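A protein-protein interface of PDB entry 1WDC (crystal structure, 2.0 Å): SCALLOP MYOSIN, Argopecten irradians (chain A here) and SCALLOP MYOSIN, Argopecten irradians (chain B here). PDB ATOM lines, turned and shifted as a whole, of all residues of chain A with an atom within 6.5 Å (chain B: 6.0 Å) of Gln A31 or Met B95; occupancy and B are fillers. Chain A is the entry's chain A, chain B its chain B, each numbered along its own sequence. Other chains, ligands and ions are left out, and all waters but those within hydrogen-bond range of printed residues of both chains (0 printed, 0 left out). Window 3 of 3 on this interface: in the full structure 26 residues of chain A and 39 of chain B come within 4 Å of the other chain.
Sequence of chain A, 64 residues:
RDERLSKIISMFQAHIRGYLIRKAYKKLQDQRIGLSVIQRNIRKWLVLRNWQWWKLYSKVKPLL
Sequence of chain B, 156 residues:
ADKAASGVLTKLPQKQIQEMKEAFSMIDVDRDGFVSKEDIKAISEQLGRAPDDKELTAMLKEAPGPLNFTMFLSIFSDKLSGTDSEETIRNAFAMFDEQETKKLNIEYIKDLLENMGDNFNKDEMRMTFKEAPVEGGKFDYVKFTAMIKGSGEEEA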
ATOM      1  N   LYS A  26      -5.295 -12.791  22.017  1.00  0.00           N
ATOM      2  CA  LYS A  26      -6.463 -13.436  22.566  1.00  0.00           C
ATOM      3  C   LYS A  26      -7.508 -12.441  23.027  1.00  0.00           C
ATOM      4  O   LYS A  26      -8.707 -12.727  23.009  1.00  0.00           O
ATOM      5  CB  LYS A  26      -6.080 -14.362  23.720  1.00  0.00           C
ATOM      6  CG  LYS A  26      -5.489 -15.727  23.279  1.00  0.00           C
ATOM      7  CD  LYS A  26      -3.999 -15.629  22.862  1.00  0.00           C
ATOM      8  CE  LYS A  26      -3.491 -16.942  22.225  1.00  0.00           C
ATOM      9  NZ  LYS A  26      -2.043 -16.866  21.794  1.00  0.00           N
ATOM     10  N   LYS A  27      -7.074 -11.237  23.357  1.00  0.00           N
ATOM     11  CA  LYS A  27      -8.016 -10.206  23.787  1.00  0.00           C
ATOM     12  C   LYS A  27      -8.768  -9.570  22.596  1.00  0.00           C
ATOM     13  O   LYS A  27      -9.924  -9.189  22.707  1.00  0.00           O
ATOM     14  CB  LYS A  27      -7.287  -9.124  24.591  1.00  0.00           C
ATOM     15  CG  LYS A  27      -8.184  -8.435  25.569  1.00  0.00           C
ATOM     16  CD  LYS A  27      -7.693  -7.038  25.877  1.00  0.00           C
ATOM     17  CE  LYS A  27      -8.266  -6.512  27.208  1.00  0.00           C
ATOM     18  NZ  LYS A  27      -7.418  -5.392  27.737  1.00  0.00           N
ATOM     19  N   LEU A  28      -8.068  -9.381  21.489  1.00  0.00           N
ATOM     20  CA  LEU A  28      -8.688  -8.986  20.251  1.00  0.00           C
ATOM     21  C   LEU A  28      -9.799  -9.978  19.862  1.00  0.00           C
ATOM     22  O   LEU A  28     -10.871  -9.581  19.452  1.00  0.00           O
ATOM     23  CB  LEU A  28      -7.640  -8.953  19.152  1.00  0.00           C
ATOM     24  CG  LEU A  28      -6.677  -7.786  19.039  1.00  0.00           C
ATOM     25  CD1 LEU A  28      -6.086  -7.820  17.628  1.00  0.00           C
ATOM     26  CD2 LEU A  28      -7.386  -6.476  19.277  1.00  0.00           C
ATOM     27  N   GLN A  29      -9.510 -11.262  19.911  1.00  0.00           N
ATOM     28  CA  GLN A  29     -10.483 -12.264  19.481  1.00  0.00           C
ATOM     29  C   GLN A  29     -11.730 -12.242  20.359  1.00  0.00           C
ATOM     30  O   GLN A  29     -12.846 -12.415  19.864  1.00  0.00           O
ATOM     31  CB  GLN A  29      -9.884 -13.674  19.515  1.00  0.00           C
ATOM     32  CG  GLN A  29      -8.801 -13.963  18.497  1.00  0.00           C
ATOM     33  CD  GLN A  29      -8.270 -15.395  18.598  1.00  0.00           C
ATOM     34  OE1 GLN A  29      -7.810 -15.859  19.656  1.00  0.00           O
ATOM     35  NE2 GLN A  29      -8.277 -16.083  17.473  1.00  0.00           N
ATOM     36  N   ASP A  30     -11.526 -12.119  21.670  1.00  0.00           N
ATOM     37  CA  ASP A  30     -12.640 -12.148  22.606  1.00  0.00           C
ATOM     38  C   ASP A  30     -13.464 -10.929  22.308  1.00  0.00           C
ATOM     39  O   ASP A  30     -14.683 -10.993  22.368  1.00  0.00           O
ATOM     40  CB  ASP A  30     -12.178 -12.093  24.069  1.00  0.00           C
ATOM     41  CG  ASP A  30     -11.530 -13.377  24.528  1.00  0.00           C
ATOM     42  OD1 ASP A  30     -11.909 -14.444  24.034  1.00  0.00           O
ATOM     43  OD2 ASP A  30     -10.624 -13.340  25.381  1.00  0.00           O
ATOM     44  N   GLN A  31     -12.795  -9.822  21.988  1.00  0.00           N
ATOM     45  CA  GLN A  31     -13.446  -8.534  21.882  1.00  0.00           C
ATOM     46  C   GLN A  31     -14.143  -8.402  20.577  1.00  0.00           C
ATOM     47  O   GLN A  31     -15.097  -7.651  20.466  1.00  0.00           O
ATOM     48  CB  GLN A  31     -12.458  -7.408  22.001  1.00  0.00           C
ATOM     49  CG  GLN A  31     -12.203  -6.998  23.445  1.00  0.00           C
ATOM     50  CD  GLN A  31     -11.118  -5.940  23.561  1.00  0.00           C
ATOM     51  OE1 GLN A  31     -10.300  -5.751  22.653  1.00  0.00           O
ATOM     52  NE2 GLN A  31     -11.144  -5.210  24.653  1.00  0.00           N
ATOM     53  N   ARG A  32     -13.625  -9.076  19.568  1.00  0.00           N
ATOM     54  CA  ARG A  32     -14.340  -9.185  18.315  1.00  0.00           C
ATOM     55  C   ARG A  32     -15.740  -9.741  18.535  1.00  0.00           C
ATOM     56  O   ARG A  32     -16.699  -9.253  17.949  1.00  0.00           O
ATOM     57  CB  ARG A  32     -13.606 -10.097  17.350  1.00  0.00           C
ATOM     58  CG  ARG A  32     -14.259 -10.122  15.979  1.00  0.00           C
ATOM     59  CD  ARG A  32     -14.459 -11.504  15.488  1.00  0.00           C
ATOM     60  NE  ARG A  32     -13.269 -12.010  14.826  1.00  0.00           N
ATOM     61  CZ  ARG A  32     -12.602 -13.094  15.214  1.00  0.00           C
ATOM     62  NH1 ARG A  32     -12.860 -13.680  16.400  1.00  0.00           N
ATOM     63  NH2 ARG A  32     -11.615 -13.536  14.449  1.00  0.00           N
ATOM     64  N   ILE A  33     -15.834 -10.764  19.387  1.00  0.00           N
ATOM     65  CA  ILE A  33     -17.104 -11.359  19.773  1.00  0.00           C
ATOM     66  C   ILE A  33     -17.979 -10.355  20.502  1.00  0.00           C
ATOM     67  O   ILE A  33     -19.157 -10.192  20.187  1.00  0.00           O
ATOM     68  CB  ILE A  33     -16.853 -12.594  20.648  1.00  0.00           C
ATOM     69  CG1 ILE A  33     -16.373 -13.715  19.740  1.00  0.00           C
ATOM     70  CG2 ILE A  33     -18.098 -12.993  21.503  1.00  0.00           C
ATOM     71  CD1 ILE A  33     -15.832 -14.915  20.508  1.00  0.00           C
ATOM     72  N   GLY A  34     -17.409  -9.668  21.472  1.00  0.00           N
ATOM     73  CA  GLY A  34     -18.162  -8.631  22.138  1.00  0.00           C
ATOM     74  C   GLY A  34     -18.692  -7.520  21.255  1.00  0.00           C
ATOM     75  O   GLY A  34     -19.804  -7.111  21.492  1.00  0.00           O
ATOM     76  N   LEU A  35     -17.897  -6.996  20.312  1.00  0.00           N
ATOM     77  CA  LEU A  35     -18.286  -5.844  19.508  1.00  0.00           C
ATOM     78  C   LEU A  35     -19.316  -6.243  18.440  1.00  0.00           C
ATOM     79  O   LEU A  35     -20.161  -5.433  18.047  1.00  0.00           O
ATOM     80  CB  LEU A  35     -17.068  -5.228  18.819  1.00  0.00           C
ATOM     81  CG  LEU A  35     -17.408  -4.036  17.936  1.00  0.00           C
ATOM     82  CD1 LEU A  35     -18.109  -2.975  18.776  1.00  0.00           C
ATOM     83  CD2 LEU A  35     -16.206  -3.420  17.279  1.00  0.00           C
ATOM     84  N   SER A  36     -19.248  -7.502  18.001  1.00  0.00           N
ATOM     85  CA  SER A  36     -20.223  -8.084  17.101  1.00  0.00           C
ATOM     86  C   SER A  36     -21.551  -8.221  17.790  1.00  0.00           C
ATOM     87  O   SER A  36     -22.563  -7.783  17.258  1.00  0.00           O
ATOM     88  CB  SER A  36     -19.757  -9.450  16.642  1.00  0.00           C
ATOM     89  OG  SER A  36     -18.664  -9.325  15.755  1.00  0.00           O
ATOM     90  N   ARG B  90     -24.958  -7.197  28.010  1.00  0.00           N
ATOM     91  CA  ARG B  90     -24.209  -6.507  29.056  1.00  0.00           C
ATOM     92  C   ARG B  90     -22.743  -6.976  29.225  1.00  0.00           C
ATOM     93  O   ARG B  90     -21.831  -6.147  29.336  1.00  0.00           O
ATOM     94  CB  ARG B  90     -24.948  -6.616  30.374  1.00  0.00           C
ATOM     95  CG  ARG B  90     -24.595  -5.498  31.312  1.00  0.00           C
ATOM     96  CD  ARG B  90     -25.205  -5.732  32.667  1.00  0.00           C
ATOM     97  NE  ARG B  90     -26.519  -6.362  32.591  1.00  0.00           N
ATOM     98  CZ  ARG B  90     -26.768  -7.577  33.061  1.00  0.00           C
ATOM     99  NH1 ARG B  90     -25.764  -8.368  33.428  1.00  0.00           N
ATOM    100  NH2 ARG B  90     -28.007  -8.027  33.096  1.00  0.00           N
ATOM    101  N   ASN B  91     -22.509  -8.283  29.107  1.00  0.00           N
ATOM    102  CA  ASN B  91     -21.159  -8.818  29.151  1.00  0.00           C
ATOM    103  C   ASN B  91     -20.312  -8.465  27.981  1.00  0.00           C
ATOM    104  O   ASN B  91     -19.095  -8.466  28.111  1.00  0.00           O
ATOM    105  CB  ASN B  91     -21.166 -10.329  29.293  1.00  0.00           C
ATOM    106  CG  ASN B  91     -21.588 -10.776  30.661  1.00  0.00           C
ATOM    107  OD1 ASN B  91     -21.960 -11.930  30.866  1.00  0.00           O
ATOM    108  ND2 ASN B  91     -21.573  -9.860  31.609  1.00  0.00           N
ATOM    109  N   ALA B  92     -20.914  -8.280  26.805  1.00  0.00           N
ATOM    110  CA  ALA B  92     -20.154  -7.888  25.621  1.00  0.00           C
ATOM    111  C   ALA B  92     -19.581  -6.498  25.811  1.00  0.00           C
ATOM    112  O   ALA B  92     -18.451  -6.250  25.438  1.00  0.00           O
ATOM    113  CB  ALA B  92     -21.030  -7.926  24.358  1.00  0.00           C
ATOM    114  N   PHE B  93     -20.389  -5.583  26.348  1.00  0.00           N
ATOM    115  CA  PHE B  93     -19.990  -4.188  26.660  1.00  0.00           C
ATOM    116  C   PHE B  93     -18.868  -4.171  27.739  1.00  0.00           C
ATOM    117  O   PHE B  93     -17.917  -3.362  27.683  1.00  0.00           O
ATOM    118  CB  PHE B  93     -21.217  -3.397  27.200  1.00  0.00           C
ATOM    119  CG  PHE B  93     -22.109  -2.752  26.122  1.00  0.00           C
ATOM    120  CD1 PHE B  93     -21.633  -1.728  25.299  1.00  0.00           C
ATOM    121  CD2 PHE B  93     -23.465  -3.074  26.034  1.00  0.00           C
ATOM    122  CE1 PHE B  93     -22.482  -1.027  24.421  1.00  0.00           C
ATOM    123  CE2 PHE B  93     -24.325  -2.366  25.143  1.00  0.00           C
ATOM    124  CZ  PHE B  93     -23.823  -1.349  24.346  1.00  0.00           C
ATOM    125  N   ALA B  94     -19.046  -5.035  28.741  1.00  0.00           N
ATOM    126  CA  ALA B  94     -18.163  -5.157  29.878  1.00  0.00           C
ATOM    127  C   ALA B  94     -16.771  -5.612  29.504  1.00  0.00           C
ATOM    128  O   ALA B  94     -15.807  -5.196  30.135  1.00  0.00           O
ATOM    129  CB  ALA B  94     -18.762  -6.076  30.883  1.00  0.00           C
ATOM    130  N   MET B  95     -16.631  -6.304  28.378  1.00  0.00           N
ATOM    131  CA  MET B  95     -15.293  -6.587  27.849  1.00  0.00           C
ATOM    132  C   MET B  95     -14.465  -5.323  27.620  1.00  0.00           C
ATOM    133  O   MET B  95     -13.293  -5.391  27.249  1.00  0.00           O
ATOM    134  CB  MET B  95     -15.398  -7.325  26.527  1.00  0.00           C
ATOM    135  CG  MET B  95     -16.206  -8.563  26.618  1.00  0.00           C
ATOM    136  SD  MET B  95     -15.939  -9.397  25.123  1.00  0.00           S
ATOM    137  CE  MET B  95     -16.886 -10.925  25.367  1.00  0.00           C
ATOM    138  N   PHE B  96     -15.142  -4.190  27.554  1.00  0.00           N
ATOM    139  CA  PHE B  96     -14.455  -2.961  27.202  1.00  0.00           C
ATOM    140  C   PHE B  96     -14.379  -2.062  28.423  1.00  0.00           C
ATOM    141  O   PHE B  96     -14.016  -0.919  28.311  1.00  0.00           O
ATOM    142  CB  PHE B  96     -15.200  -2.269  26.062  1.00  0.00           C
ATOM    143  CG  PHE B  96     -15.258  -3.078  24.802  1.00  0.00           C
ATOM    144  CD1 PHE B  96     -16.282  -3.999  24.597  1.00  0.00           C
ATOM    145  CD2 PHE B  96     -14.275  -2.952  23.832  1.00  0.00           C
ATOM    146  CE1 PHE B  96     -16.320  -4.810  23.437  1.00  0.00           C
ATOM    147  CE2 PHE B  96     -14.305  -3.753  22.663  1.00  0.00           C
ATOM    148  CZ  PHE B  96     -15.344  -4.698  22.479  1.00  0.00           C
ATOM    149  N   ASP B  97     -14.780  -2.602  29.563  1.00  0.00           N
ATOM    150  CA  ASP B  97     -14.833  -1.901  30.840  1.00  0.00           C
ATOM    151  C   ASP B  97     -14.049  -2.708  31.918  1.00  0.00           C
ATOM    152  O   ASP B  97     -14.635  -3.295  32.815  1.00  0.00           O
ATOM    153  CB  ASP B  97     -16.315  -1.749  31.251  1.00  0.00           C
ATOM    154  CG  ASP B  97     -16.503  -1.072  32.592  1.00  0.00           C
ATOM    155  OD1 ASP B  97     -15.793  -0.082  32.864  1.00  0.00           O
ATOM    156  OD2 ASP B  97     -17.389  -1.504  33.360  1.00  0.00           O
ATOM    157  N   GLU B  98     -12.726  -2.710  31.855  1.00  0.00           N
ATOM    158  CA  GLU B  98     -11.930  -3.627  32.667  1.00  0.00           C
ATOM    159  C   GLU B  98     -11.966  -3.378  34.179  1.00  0.00           C
ATOM    160  O   GLU B  98     -11.908  -4.303  34.967  1.00  0.00           O
ATOM    161  CB  GLU B  98     -10.488  -3.613  32.163  1.00  0.00           C
ATOM    162  CG  GLU B  98     -10.149  -2.465  31.179  1.00  0.00           C
ATOM    163  CD  GLU B  98     -10.780  -2.603  29.758  1.00  0.00           C
ATOM    164  OE1 GLU B  98     -10.797  -3.731  29.184  1.00  0.00           O
ATOM    165  OE2 GLU B  98     -11.171  -1.548  29.190  1.00  0.00           O
ATOM    166  N   TYR B 108     -15.146   6.675  23.419  1.00  0.00           N
ATOM    167  CA  TYR B 108     -14.678   5.321  23.185  1.00  0.00           C
ATOM    168  C   TYR B 108     -15.769   4.441  22.505  1.00  0.00           C
ATOM    169  O   TYR B 108     -15.542   3.920  21.417  1.00  0.00           O
ATOM    170  CB  TYR B 108     -14.237   4.732  24.519  1.00  0.00           C
ATOM    171  CG  TYR B 108     -13.620   3.370  24.397  1.00  0.00           C
ATOM    172  CD1 TYR B 108     -12.825   3.021  23.285  1.00  0.00           C
ATOM    173  CD2 TYR B 108     -13.788   2.431  25.409  1.00  0.00           C
ATOM    174  CE1 TYR B 108     -12.227   1.749  23.197  1.00  0.00           C
ATOM    175  CE2 TYR B 108     -13.176   1.179  25.342  1.00  0.00           C
ATOM    176  CZ  TYR B 108     -12.411   0.840  24.241  1.00  0.00           C
ATOM    177  OH  TYR B 108     -11.903  -0.439  24.194  1.00  0.00           O
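The backbone carbonyl oxygen of Lys A27 lies close to the side-chain amide oxygen of Gln A31 (3.5 Å).
Among the printed residues, merely in contact across the chains: Gln A31 with Phe B96 (3.6 Å), Gly A34 with Ala B92 (3.2 Å) and Gly A34 with Met B95 (3.8 Å).
The backbone carbonyl oxygen of Met B95 is in hydrogen-bond range of the side-chain amide nitrogen of Gln A31, at 3.4 Å. The side-chain sulfur (SD) of Met B95 sits close to the backbone carbonyl oxygen (O) of Asp A30.
Met B95 touches just these residues of chain A: Asp A30, Gln A31 and Gly A34. Printed residues of chain A within 4 Å of Ala B92: Gly A34 (3.2 Å). Of the printed residues of chain A, Phe B96 touches Gln A31. Of the printed residues of chain B, Gly A34 touches Ala B92 and Met B95. Lys A26 touches none of the printed residues of chain B.
Printed residues of chain B that touch a printed residue of chain A: Ala B92, Met B95 and Phe B96. Hydrophobic or aromatic side chains of chain B within 4 Å of the printed part of chain A: Ala B92, Met B95 and Phe B96. Among the printed residues, 5 pairs touch across the chains.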
